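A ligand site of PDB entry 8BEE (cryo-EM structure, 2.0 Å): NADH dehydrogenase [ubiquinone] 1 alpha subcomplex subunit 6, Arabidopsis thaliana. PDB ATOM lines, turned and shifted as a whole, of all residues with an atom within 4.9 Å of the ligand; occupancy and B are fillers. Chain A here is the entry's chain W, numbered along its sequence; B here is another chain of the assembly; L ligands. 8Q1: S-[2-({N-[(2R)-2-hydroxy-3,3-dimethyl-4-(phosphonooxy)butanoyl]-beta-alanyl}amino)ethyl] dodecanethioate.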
ATOM      1  N   ARG A  23      -3.767  10.937 -34.438  1.00  0.00           N
ATOM      2  CA  ARG A  23      -2.994  12.015 -35.040  1.00  0.00           C
ATOM      3  C   ARG A  23      -3.894  13.172 -35.463  1.00  0.00           C
ATOM      4  O   ARG A  23      -3.537  14.343 -35.315  1.00  0.00           O
ATOM      5  CB  ARG A  23      -2.191  11.494 -36.235  1.00  0.00           C
ATOM      6  CG  ARG A  23      -1.331  12.534 -36.918  1.00  0.00           C
ATOM      7  CD  ARG A  23      -0.169  11.907 -37.679  1.00  0.00           C
ATOM      8  NE  ARG A  23      -0.441  10.548 -38.117  1.00  0.00           N
ATOM      9  CZ  ARG A  23       0.275   9.486 -37.772  1.00  0.00           C
ATOM     10  NH1 ARG A  23       1.315   9.599 -36.946  1.00  0.00           N
ATOM     11  NH2 ARG A  23      -0.053   8.291 -38.242  1.00  0.00           N
ATOM     12  N   VAL A  26      -4.612  15.088 -32.491  1.00  0.00           N
ATOM     13  CA  VAL A  26      -3.424  15.882 -32.147  1.00  0.00           C
ATOM     14  C   VAL A  26      -3.403  17.168 -32.968  1.00  0.00           C
ATOM     15  O   VAL A  26      -3.135  18.258 -32.440  1.00  0.00           O
ATOM     16  CB  VAL A  26      -2.129  15.072 -32.370  1.00  0.00           C
ATOM     17  CG1 VAL A  26      -0.918  15.975 -32.204  1.00  0.00           C
ATOM     18  CG2 VAL A  26      -2.037  13.911 -31.425  1.00  0.00           C
ATOM     19  N   PHE A  27      -3.660  17.066 -34.274  1.00  0.00           N
ATOM     20  CA  PHE A  27      -3.622  18.244 -35.127  1.00  0.00           C
ATOM     21  C   PHE A  27      -4.721  19.237 -34.713  1.00  0.00           C
ATOM     22  O   PHE A  27      -4.473  20.454 -34.684  1.00  0.00           O
ATOM     23  CB  PHE A  27      -3.768  17.850 -36.592  1.00  0.00           C
ATOM     24  CG  PHE A  27      -2.518  17.264 -37.191  1.00  0.00           C
ATOM     25  CD1 PHE A  27      -1.333  17.246 -36.472  1.00  0.00           C
ATOM     26  CD2 PHE A  27      -2.518  16.737 -38.468  1.00  0.00           C
ATOM     27  CE1 PHE A  27      -0.182  16.715 -37.012  1.00  0.00           C
ATOM     28  CE2 PHE A  27      -1.368  16.201 -39.025  1.00  0.00           C
ATOM     29  CZ  PHE A  27      -0.194  16.182 -38.286  1.00  0.00           C
ATOM     30  N   PHE A  29      -5.967  19.600 -31.673  1.00  0.00           N
ATOM     31  CA  PHE A  29      -5.552  20.241 -30.429  1.00  0.00           C
ATOM     32  C   PHE A  29      -4.489  21.296 -30.687  1.00  0.00           C
ATOM     33  O   PHE A  29      -4.497  22.363 -30.061  1.00  0.00           O
ATOM     34  CB  PHE A  29      -5.025  19.210 -29.432  1.00  0.00           C
ATOM     35  CG  PHE A  29      -4.223  19.817 -28.325  1.00  0.00           C
ATOM     36  CD1 PHE A  29      -4.866  20.472 -27.284  1.00  0.00           C
ATOM     37  CD2 PHE A  29      -2.839  19.781 -28.335  1.00  0.00           C
ATOM     38  CE1 PHE A  29      -4.140  21.053 -26.260  1.00  0.00           C
ATOM     39  CE2 PHE A  29      -2.115  20.358 -27.327  1.00  0.00           C
ATOM     40  CZ  PHE A  29      -2.767  20.998 -26.288  1.00  0.00           C
ATOM     41  N   ALA A  33      -4.727  25.202 -29.727  1.00  0.00           N
ATOM     42  CA  ALA A  33      -3.743  25.836 -28.854  1.00  0.00           C
ATOM     43  C   ALA A  33      -3.104  27.045 -29.525  1.00  0.00           C
ATOM     44  O   ALA A  33      -2.928  28.092 -28.891  1.00  0.00           O
ATOM     45  CB  ALA A  33      -2.666  24.821 -28.457  1.00  0.00           C
ATOM     46  N   ILE A  40      -3.763  34.818 -24.997  1.00  0.00           N
ATOM     47  CA  ILE A  40      -2.771  34.633 -23.941  1.00  0.00           C
ATOM     48  C   ILE A  40      -1.822  35.825 -23.892  1.00  0.00           C
ATOM     49  O   ILE A  40      -1.457  36.302 -22.813  1.00  0.00           O
ATOM     50  CB  ILE A  40      -2.017  33.307 -24.151  1.00  0.00           C
ATOM     51  CG1 ILE A  40      -2.937  32.137 -23.799  1.00  0.00           C
ATOM     52  CG2 ILE A  40      -0.741  33.276 -23.326  1.00  0.00           C
ATOM     53  CD1 ILE A  40      -2.511  30.821 -24.381  1.00  0.00           C
ATOM     54  N   ILE A  59       4.735  25.013 -27.999  1.00  0.00           N
ATOM     55  CA  ILE A  59       3.666  24.025 -28.116  1.00  0.00           C
ATOM     56  C   ILE A  59       4.089  22.889 -29.040  1.00  0.00           C
ATOM     57  O   ILE A  59       3.925  21.702 -28.723  1.00  0.00           O
ATOM     58  CB  ILE A  59       2.361  24.678 -28.599  1.00  0.00           C
ATOM     59  CG1 ILE A  59       1.888  25.738 -27.619  1.00  0.00           C
ATOM     60  CG2 ILE A  59       1.275  23.643 -28.780  1.00  0.00           C
ATOM     61  CD1 ILE A  59       0.715  26.541 -28.133  1.00  0.00           C
ATOM     62  N   GLN A  62       6.617  20.623 -27.419  1.00  0.00           N
ATOM     63  CA  GLN A  62       5.961  19.695 -26.508  1.00  0.00           C
ATOM     64  C   GLN A  62       5.328  18.537 -27.258  1.00  0.00           C
ATOM     65  O   GLN A  62       5.396  17.381 -26.825  1.00  0.00           O
ATOM     66  CB  GLN A  62       4.903  20.426 -25.666  1.00  0.00           C
ATOM     67  CG  GLN A  62       5.468  21.224 -24.504  1.00  0.00           C
ATOM     68  CD  GLN A  62       6.034  20.359 -23.384  1.00  0.00           C
ATOM     69  OE1 GLN A  62       5.936  19.133 -23.429  1.00  0.00           O
ATOM     70  NE2 GLN A  62       6.656  20.998 -22.391  1.00  0.00           N
ATOM     71  N   ILE A  63       4.710  18.826 -28.412  1.00  0.00           N
ATOM     72  CA  ILE A  63       4.128  17.758 -29.222  1.00  0.00           C
ATOM     73  C   ILE A  63       5.214  16.839 -29.765  1.00  0.00           C
ATOM     74  O   ILE A  63       5.022  15.617 -29.870  1.00  0.00           O
ATOM     75  CB  ILE A  63       3.266  18.362 -30.351  1.00  0.00           C
ATOM     76  CG1 ILE A  63       2.062  19.086 -29.772  1.00  0.00           C
ATOM     77  CG2 ILE A  63       2.833  17.282 -31.333  1.00  0.00           C
ATOM     78  CD1 ILE A  63       1.167  19.719 -30.809  1.00  0.00           C
ATOM     79  N   ARG A  64       6.376  17.394 -30.109  1.00  0.00           N
ATOM     80  CA  ARG A  64       7.432  16.606 -30.742  1.00  0.00           C
ATOM     81  C   ARG A  64       8.153  15.723 -29.743  1.00  0.00           C
ATOM     82  O   ARG A  64       8.559  14.611 -30.070  1.00  0.00           O
ATOM     83  CB  ARG A  64       8.423  17.532 -31.450  1.00  0.00           C
ATOM     84  CG  ARG A  64       7.886  18.164 -32.699  1.00  0.00           C
ATOM     85  CD  ARG A  64       8.834  17.989 -33.862  1.00  0.00           C
ATOM     86  NE  ARG A  64       8.340  18.657 -35.052  1.00  0.00           N
ATOM     87  CZ  ARG A  64       8.098  18.047 -36.199  1.00  0.00           C
ATOM     88  NH1 ARG A  64       8.316  16.749 -36.353  1.00  0.00           N
ATOM     89  NH2 ARG A  64       7.646  18.752 -37.229  1.00  0.00           N
ATOM     90  N   ASN A  66       6.979  14.036 -27.513  1.00  0.00           N
ATOM     91  CA  ASN A  66       6.186  12.834 -27.332  1.00  0.00           C
ATOM     92  C   ASN A  66       5.916  12.116 -28.650  1.00  0.00           C
ATOM     93  O   ASN A  66       4.977  11.324 -28.745  1.00  0.00           O
ATOM     94  CB  ASN A  66       4.856  13.162 -26.651  1.00  0.00           C
ATOM     95  CG  ASN A  66       5.018  13.518 -25.188  1.00  0.00           C
ATOM     96  OD1 ASN A  66       4.610  14.595 -24.755  1.00  0.00           O
ATOM     97  ND2 ASN A  66       5.618  12.620 -24.417  1.00  0.00           N
ATOM     98  N   ALA A  67       6.727  12.370 -29.674  1.00  0.00           N
ATOM     99  CA  ALA A  67       6.494  11.772 -30.976  1.00  0.00           C
ATOM    100  C   ALA A  67       6.769  10.274 -31.016  1.00  0.00           C
ATOM    101  O   ALA A  67       6.406   9.627 -31.992  1.00  0.00           O
ATOM    102  CB  ALA A  67       7.342  12.478 -32.037  1.00  0.00           C
ATOM    103  N   ILE A  69       5.455   8.100 -28.940  1.00  0.00           N
ATOM    104  CA  ILE A  69       4.340   7.350 -28.369  1.00  0.00           C
ATOM    105  C   ILE A  69       3.612   6.611 -29.479  1.00  0.00           C
ATOM    106  O   ILE A  69       3.301   7.181 -30.530  1.00  0.00           O
ATOM    107  CB  ILE A  69       3.396   8.284 -27.613  1.00  0.00           C
ATOM    108  CG1 ILE A  69       4.080   8.856 -26.359  1.00  0.00           C
ATOM    109  CG2 ILE A  69       2.125   7.563 -27.236  1.00  0.00           C
ATOM    110  CD1 ILE A  69       4.927   7.850 -25.614  1.00  0.00           C
ATOM    111  N   ILE A  75      -1.945   8.800 -26.250  1.00  0.00           N
ATOM    112  CA  ILE A  75      -2.072  10.041 -27.010  1.00  0.00           C
ATOM    113  C   ILE A  75      -3.364  10.763 -26.658  1.00  0.00           C
ATOM    114  O   ILE A  75      -3.387  11.985 -26.486  1.00  0.00           O
ATOM    115  CB  ILE A  75      -1.982   9.734 -28.515  1.00  0.00           C
ATOM    116  CG1 ILE A  75      -0.589   9.210 -28.872  1.00  0.00           C
ATOM    117  CG2 ILE A  75      -2.322  10.969 -29.328  1.00  0.00           C
ATOM    118  CD1 ILE A  75      -0.447   8.801 -30.310  1.00  0.00           C
ATOM    119  N   LEU A  78      -2.939  12.365 -23.299  1.00  0.00           N
ATOM    120  CA  LEU A  78      -2.074  13.533 -23.398  1.00  0.00           C
ATOM    121  C   LEU A  78      -2.827  14.715 -23.998  1.00  0.00           C
ATOM    122  O   LEU A  78      -2.677  15.857 -23.552  1.00  0.00           O
ATOM    123  CB  LEU A  78      -0.826  13.201 -24.215  1.00  0.00           C
ATOM    124  CG  LEU A  78       0.207  12.293 -23.544  1.00  0.00           C
ATOM    125  CD1 LEU A  78       1.318  11.937 -24.500  1.00  0.00           C
ATOM    126  CD2 LEU A  78       0.761  12.915 -22.276  1.00  0.00           C
ATOM    127  N   ILE A  79      -3.661  14.457 -25.010  1.00  0.00           N
ATOM    128  CA  ILE A  79      -4.454  15.513 -25.618  1.00  0.00           C
ATOM    129  C   ILE A  79      -5.466  16.071 -24.627  1.00  0.00           C
ATOM    130  O   ILE A  79      -5.688  17.287 -24.552  1.00  0.00           O
ATOM    131  CB  ILE A  79      -5.154  15.003 -26.895  1.00  0.00           C
ATOM    132  CG1 ILE A  79      -4.140  14.709 -27.993  1.00  0.00           C
ATOM    133  CG2 ILE A  79      -6.163  16.015 -27.387  1.00  0.00           C
ATOM    134  CD1 ILE A  79      -4.711  13.858 -29.115  1.00  0.00           C
ATOM    135  N   GLY A  82      -3.592  18.224 -22.196  1.00  0.00           N
ATOM    136  CA  GLY A  82      -3.221  19.458 -22.852  1.00  0.00           C
ATOM    137  C   GLY A  82      -4.385  20.429 -22.975  1.00  0.00           C
ATOM    138  O   GLY A  82      -4.227  21.631 -22.771  1.00  0.00           O
ATOM    139  N   GLU A  85      -4.996  21.924 -19.522  1.00  0.00           N
ATOM    140  CA  GLU A  85      -3.980  22.918 -19.197  1.00  0.00           C
ATOM    141  C   GLU A  85      -4.174  24.207 -19.989  1.00  0.00           C
ATOM    142  O   GLU A  85      -4.031  25.304 -19.446  1.00  0.00           O
ATOM    143  CB  GLU A  85      -2.586  22.328 -19.427  1.00  0.00           C
ATOM    144  CG  GLU A  85      -1.578  23.302 -19.994  1.00  0.00           C
ATOM    145  CD  GLU A  85      -0.150  22.887 -19.699  1.00  0.00           C
ATOM    146  OE1 GLU A  85       0.118  21.678 -19.617  1.00  0.00           O
ATOM    147  OE2 GLU A  85       0.704  23.784 -19.519  1.00  0.00           O
ATOM    148  N   LEU A  86      -4.522  24.088 -21.277  1.00  0.00           N
ATOM    149  CA  LEU A  86      -4.818  25.264 -22.076  1.00  0.00           C
ATOM    150  C   LEU A  86      -6.012  26.025 -21.521  1.00  0.00           C
ATOM    151  O   LEU A  86      -5.998  27.262 -21.435  1.00  0.00           O
ATOM    152  CB  LEU A  86      -5.092  24.849 -23.519  1.00  0.00           C
ATOM    153  CG  LEU A  86      -5.504  25.949 -24.504  1.00  0.00           C
ATOM    154  CD1 LEU A  86      -4.456  27.041 -24.566  1.00  0.00           C
ATOM    155  CD2 LEU A  86      -5.781  25.364 -25.872  1.00  0.00           C
ATOM    156  N   ILE A  89      -4.973  27.854 -18.430  1.00  0.00           N
ATOM    157  CA  ILE A  89      -4.108  28.979 -18.800  1.00  0.00           C
ATOM    158  C   ILE A  89      -4.937  30.155 -19.289  1.00  0.00           C
ATOM    159  O   ILE A  89      -4.699  31.313 -18.916  1.00  0.00           O
ATOM    160  CB  ILE A  89      -3.068  28.531 -19.838  1.00  0.00           C
ATOM    161  CG1 ILE A  89      -1.838  27.963 -19.162  1.00  0.00           C
ATOM    162  CG2 ILE A  89      -2.691  29.690 -20.768  1.00  0.00           C
ATOM    163  CD1 ILE A  89      -0.917  27.232 -20.089  1.00  0.00           C
ATOM    164  N   ILE A 100       4.505  30.946 -17.730  1.00  0.00           N
ATOM    165  CA  ILE A 100       3.043  30.706 -17.995  1.00  0.00           C
ATOM    166  C   ILE A 100       2.792  29.223 -17.700  1.00  0.00           C
ATOM    167  O   ILE A 100       3.497  28.423 -18.268  1.00  0.00           O
ATOM    168  CB  ILE A 100       2.622  30.996 -19.443  1.00  0.00           C
ATOM    169  CG1 ILE A 100       2.885  32.439 -19.873  1.00  0.00           C
ATOM    170  CG2 ILE A 100       1.153  30.650 -19.623  1.00  0.00           C
ATOM    171  CD1 ILE A 100       2.873  32.604 -21.362  1.00  0.00           C
ATOM    172  N   TYR A 103       5.584  26.495 -18.385  1.00  0.00           N
ATOM    173  CA  TYR A 103       6.665  26.964 -19.289  1.00  0.00           C
ATOM    174  C   TYR A 103       7.274  28.304 -18.903  1.00  0.00           C
ATOM    175  O   TYR A 103       6.548  29.252 -18.641  1.00  0.00           O
ATOM    176  CB  TYR A 103       6.208  26.950 -20.724  1.00  0.00           C
ATOM    177  CG  TYR A 103       5.313  25.766 -20.986  1.00  0.00           C
ATOM    178  CD1 TYR A 103       5.826  24.499 -21.131  1.00  0.00           C
ATOM    179  CD2 TYR A 103       3.947  25.924 -21.007  1.00  0.00           C
ATOM    180  CE1 TYR A 103       5.001  23.402 -21.328  1.00  0.00           C
ATOM    181  CE2 TYR A 103       3.107  24.844 -21.201  1.00  0.00           C
ATOM    182  CZ  TYR A 103       3.635  23.583 -21.373  1.00  0.00           C
ATOM    183  OH  TYR A 103       2.802  22.526 -21.563  1.00  0.00           O
ATOM    184  N   ASP B  82       7.488  17.736 -42.404  1.00  0.00           N
ATOM    185  CA  ASP B  82       6.491  16.725 -42.085  1.00  0.00           C
ATOM    186  C   ASP B  82       5.114  17.365 -41.932  1.00  0.00           C
ATOM    187  O   ASP B  82       4.949  18.584 -42.031  1.00  0.00           O
ATOM    188  CB  ASP B  82       6.907  15.938 -40.842  1.00  0.00           C
ATOM    189  CG  ASP B  82       7.142  16.827 -39.631  1.00  0.00           C
ATOM    190  OD1 ASP B  82       6.468  17.868 -39.490  1.00  0.00           O
ATOM    191  OD2 ASP B  82       8.005  16.466 -38.803  1.00  0.00           O
ATOM    192  N   SER B  83       4.105  16.527 -41.681  1.00  0.00           N
ATOM    193  CA  SER B  83       2.736  17.028 -41.597  1.00  0.00           C
ATOM    194  C   SER B  83       2.574  18.006 -40.438  1.00  0.00           C
ATOM    195  O   SER B  83       1.865  19.013 -40.568  1.00  0.00           O
ATOM    196  CB  SER B  83       1.744  15.871 -41.442  1.00  0.00           C
ATOM    197  OG  SER B  83       2.192  14.944 -40.486  1.00  0.00           O
ATOM    198  N   LEU B  84       3.217  17.737 -39.310  1.00  0.00           N
ATOM    199  CA  LEU B  84       3.177  18.685 -38.195  1.00  0.00           C
ATOM    200  C   LEU B  84       3.761  20.031 -38.617  1.00  0.00           C
ATOM    201  O   LEU B  84       3.187  21.083 -38.313  1.00  0.00           O
ATOM    202  CB  LEU B  84       3.932  18.126 -36.992  1.00  0.00           C
ATOM    203  CG  LEU B  84       3.916  19.029 -35.751  1.00  0.00           C
ATOM    204  CD1 LEU B  84       2.492  19.451 -35.422  1.00  0.00           C
ATOM    205  CD2 LEU B  84       4.574  18.362 -34.563  1.00  0.00           C
HETATM  206  O4  8Q1 L   1       2.516  15.611 -26.785  1.00  0.00           O
HETATM  207  C16 8Q1 L   1       0.755  28.041 -23.650  1.00  0.00           C
HETATM  208  O3  8Q1 L   1       4.430  15.055 -38.808  1.00  0.00           O
HETATM  209  C15 8Q1 L   1       0.526  26.609 -24.071  1.00  0.00           C
HETATM  210  C14 8Q1 L   1      -0.798  26.050 -23.610  1.00  0.00           C
HETATM  211  C13 8Q1 L   1      -1.068  24.642 -24.064  1.00  0.00           C
HETATM  212  O2  8Q1 L   1       5.800  13.003 -38.261  1.00  0.00           O
HETATM  213  C12 8Q1 L   1       0.005  23.652 -23.704  1.00  0.00           C
HETATM  214  C11 8Q1 L   1      -0.285  22.242 -24.145  1.00  0.00           C
HETATM  215  C10 8Q1 L   1       0.832  21.259 -23.899  1.00  0.00           C
HETATM  216  C9  8Q1 L   1       0.553  19.867 -24.400  1.00  0.00           C
HETATM  217  C8  8Q1 L   1       1.654  18.879 -24.127  1.00  0.00           C
HETATM  218  C7  8Q1 L   1       1.424  17.495 -24.713  1.00  0.00           C
HETATM  219  C6  8Q1 L   1       1.198  17.510 -26.188  1.00  0.00           C
HETATM  220  C1  8Q1 L   1       1.457  16.179 -26.843  1.00  0.00           C
HETATM  221  C28 8Q1 L   1       3.427  14.191 -36.252  1.00  0.00           C
HETATM  222  C29 8Q1 L   1       4.308  13.665 -35.130  1.00  0.00           C
HETATM  223  C30 8Q1 L   1       5.727  14.223 -35.297  1.00  0.00           C
HETATM  224  C31 8Q1 L   1       3.761  14.157 -33.791  1.00  0.00           C
HETATM  225  C32 8Q1 L   1       4.350  12.119 -35.143  1.00  0.00           C
HETATM  226  C34 8Q1 L   1       3.205  11.454 -34.394  1.00  0.00           C
HETATM  227  C37 8Q1 L   1       2.531  10.141 -32.441  1.00  0.00           C
HETATM  228  C38 8Q1 L   1       2.643  10.680 -31.021  1.00  0.00           C
HETATM  229  C39 8Q1 L   1       1.996  12.034 -30.841  1.00  0.00           C
HETATM  230  C42 8Q1 L   1       1.613  13.935 -29.322  1.00  0.00           C
HETATM  231  C43 8Q1 L   1       0.628  13.900 -28.179  1.00  0.00           C
HETATM  232  N36 8Q1 L   1       3.519  10.741 -33.326  1.00  0.00           N
HETATM  233  N41 8Q1 L   1       2.131  12.609 -29.644  1.00  0.00           N
HETATM  234  O27 8Q1 L   1       3.447  13.263 -37.377  1.00  0.00           O
HETATM  235  O33 8Q1 L   1       5.592  11.686 -34.609  1.00  0.00           O
HETATM  236  O35 8Q1 L   1       2.046  11.605 -34.786  1.00  0.00           O
HETATM  237  O40 8Q1 L   1       1.391  12.583 -31.764  1.00  0.00           O
HETATM  238  P24 8Q1 L   1       4.438  13.553 -38.631  1.00  0.00           P
HETATM  239  S44 8Q1 L   1       0.047  15.542 -27.684  1.00  0.00           S
HETATM  240  O1  8Q1 L   1       3.813  12.818 -39.800  1.00  0.00           O
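An oxygen (O4) of the ligand lies close to the backbone carbonyl oxygen (O) of Gln 62.
Val 26 touches the ligand (CG2 to O40, 3.7 Å).
Phe 29 touches the ligand (CZ to C11, 3.5 Å).
CG1 of Ile 59 touches C15 of the ligand (3.9 Å).
Ile 63 touches the ligand (CA to O4, 3.6 Å).
NH1 of Arg 64 touches C30 of the ligand (3.8 Å).
Ile 69 touches the ligand.
CD1 of Ile 75 touches C38 of the ligand, 3.7 Å away.
Leu 86 touches the ligand (CD1 to C14, 3.9 Å).
Ile 89 touches the ligand.
Tyr 103 touches the ligand.
Asp 82 of chain B touches the ligand.
The nearest printed residue that does not touch the ligand is Glu 85 (4.05 Å).
An oxygen (O1) of the ligand lies within hydrogen-bond range of the side-chain hydroxyl of Ser 83 of chain B, at 2.8 Å.
OD1 of Asn 66 lies close to O4 of the ligand, 3.1 Å away.
The backbone NH (N) of Ser 83 of chain B lies within hydrogen-bond range of an oxygen (O3) of the ligand (3.2 Å).
N41 of the ligand is in hydrogen-bond range of O of Asn 66 (3.2 Å).
An oxygen (O3) of the ligand is in hydrogen-bond range of the backbone NH (N) of Leu 84 of chain B, at 3.0 Å.
An oxygen (O35) of the ligand is in hydrogen-bond range of the guanidinium group of Arg 23 (3.0 Å).
A nitrogen (N36) of the ligand is in hydrogen-bond range of the backbone carbonyl oxygen (O) of Ala 67.
OH of Tyr 103 sits close to OE2 of Glu 85 (3.2 Å).
The guanidinium group (NH1) of Arg 64 is in salt-bridge range of the side-chain carboxylate (OD2) of Asp 82 of chain B, 2.5 Å away.
The backbone NH (N) of Leu 84 of chain B sits close to the side-chain carboxylate (OD1) of Asp 82 of chain B.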
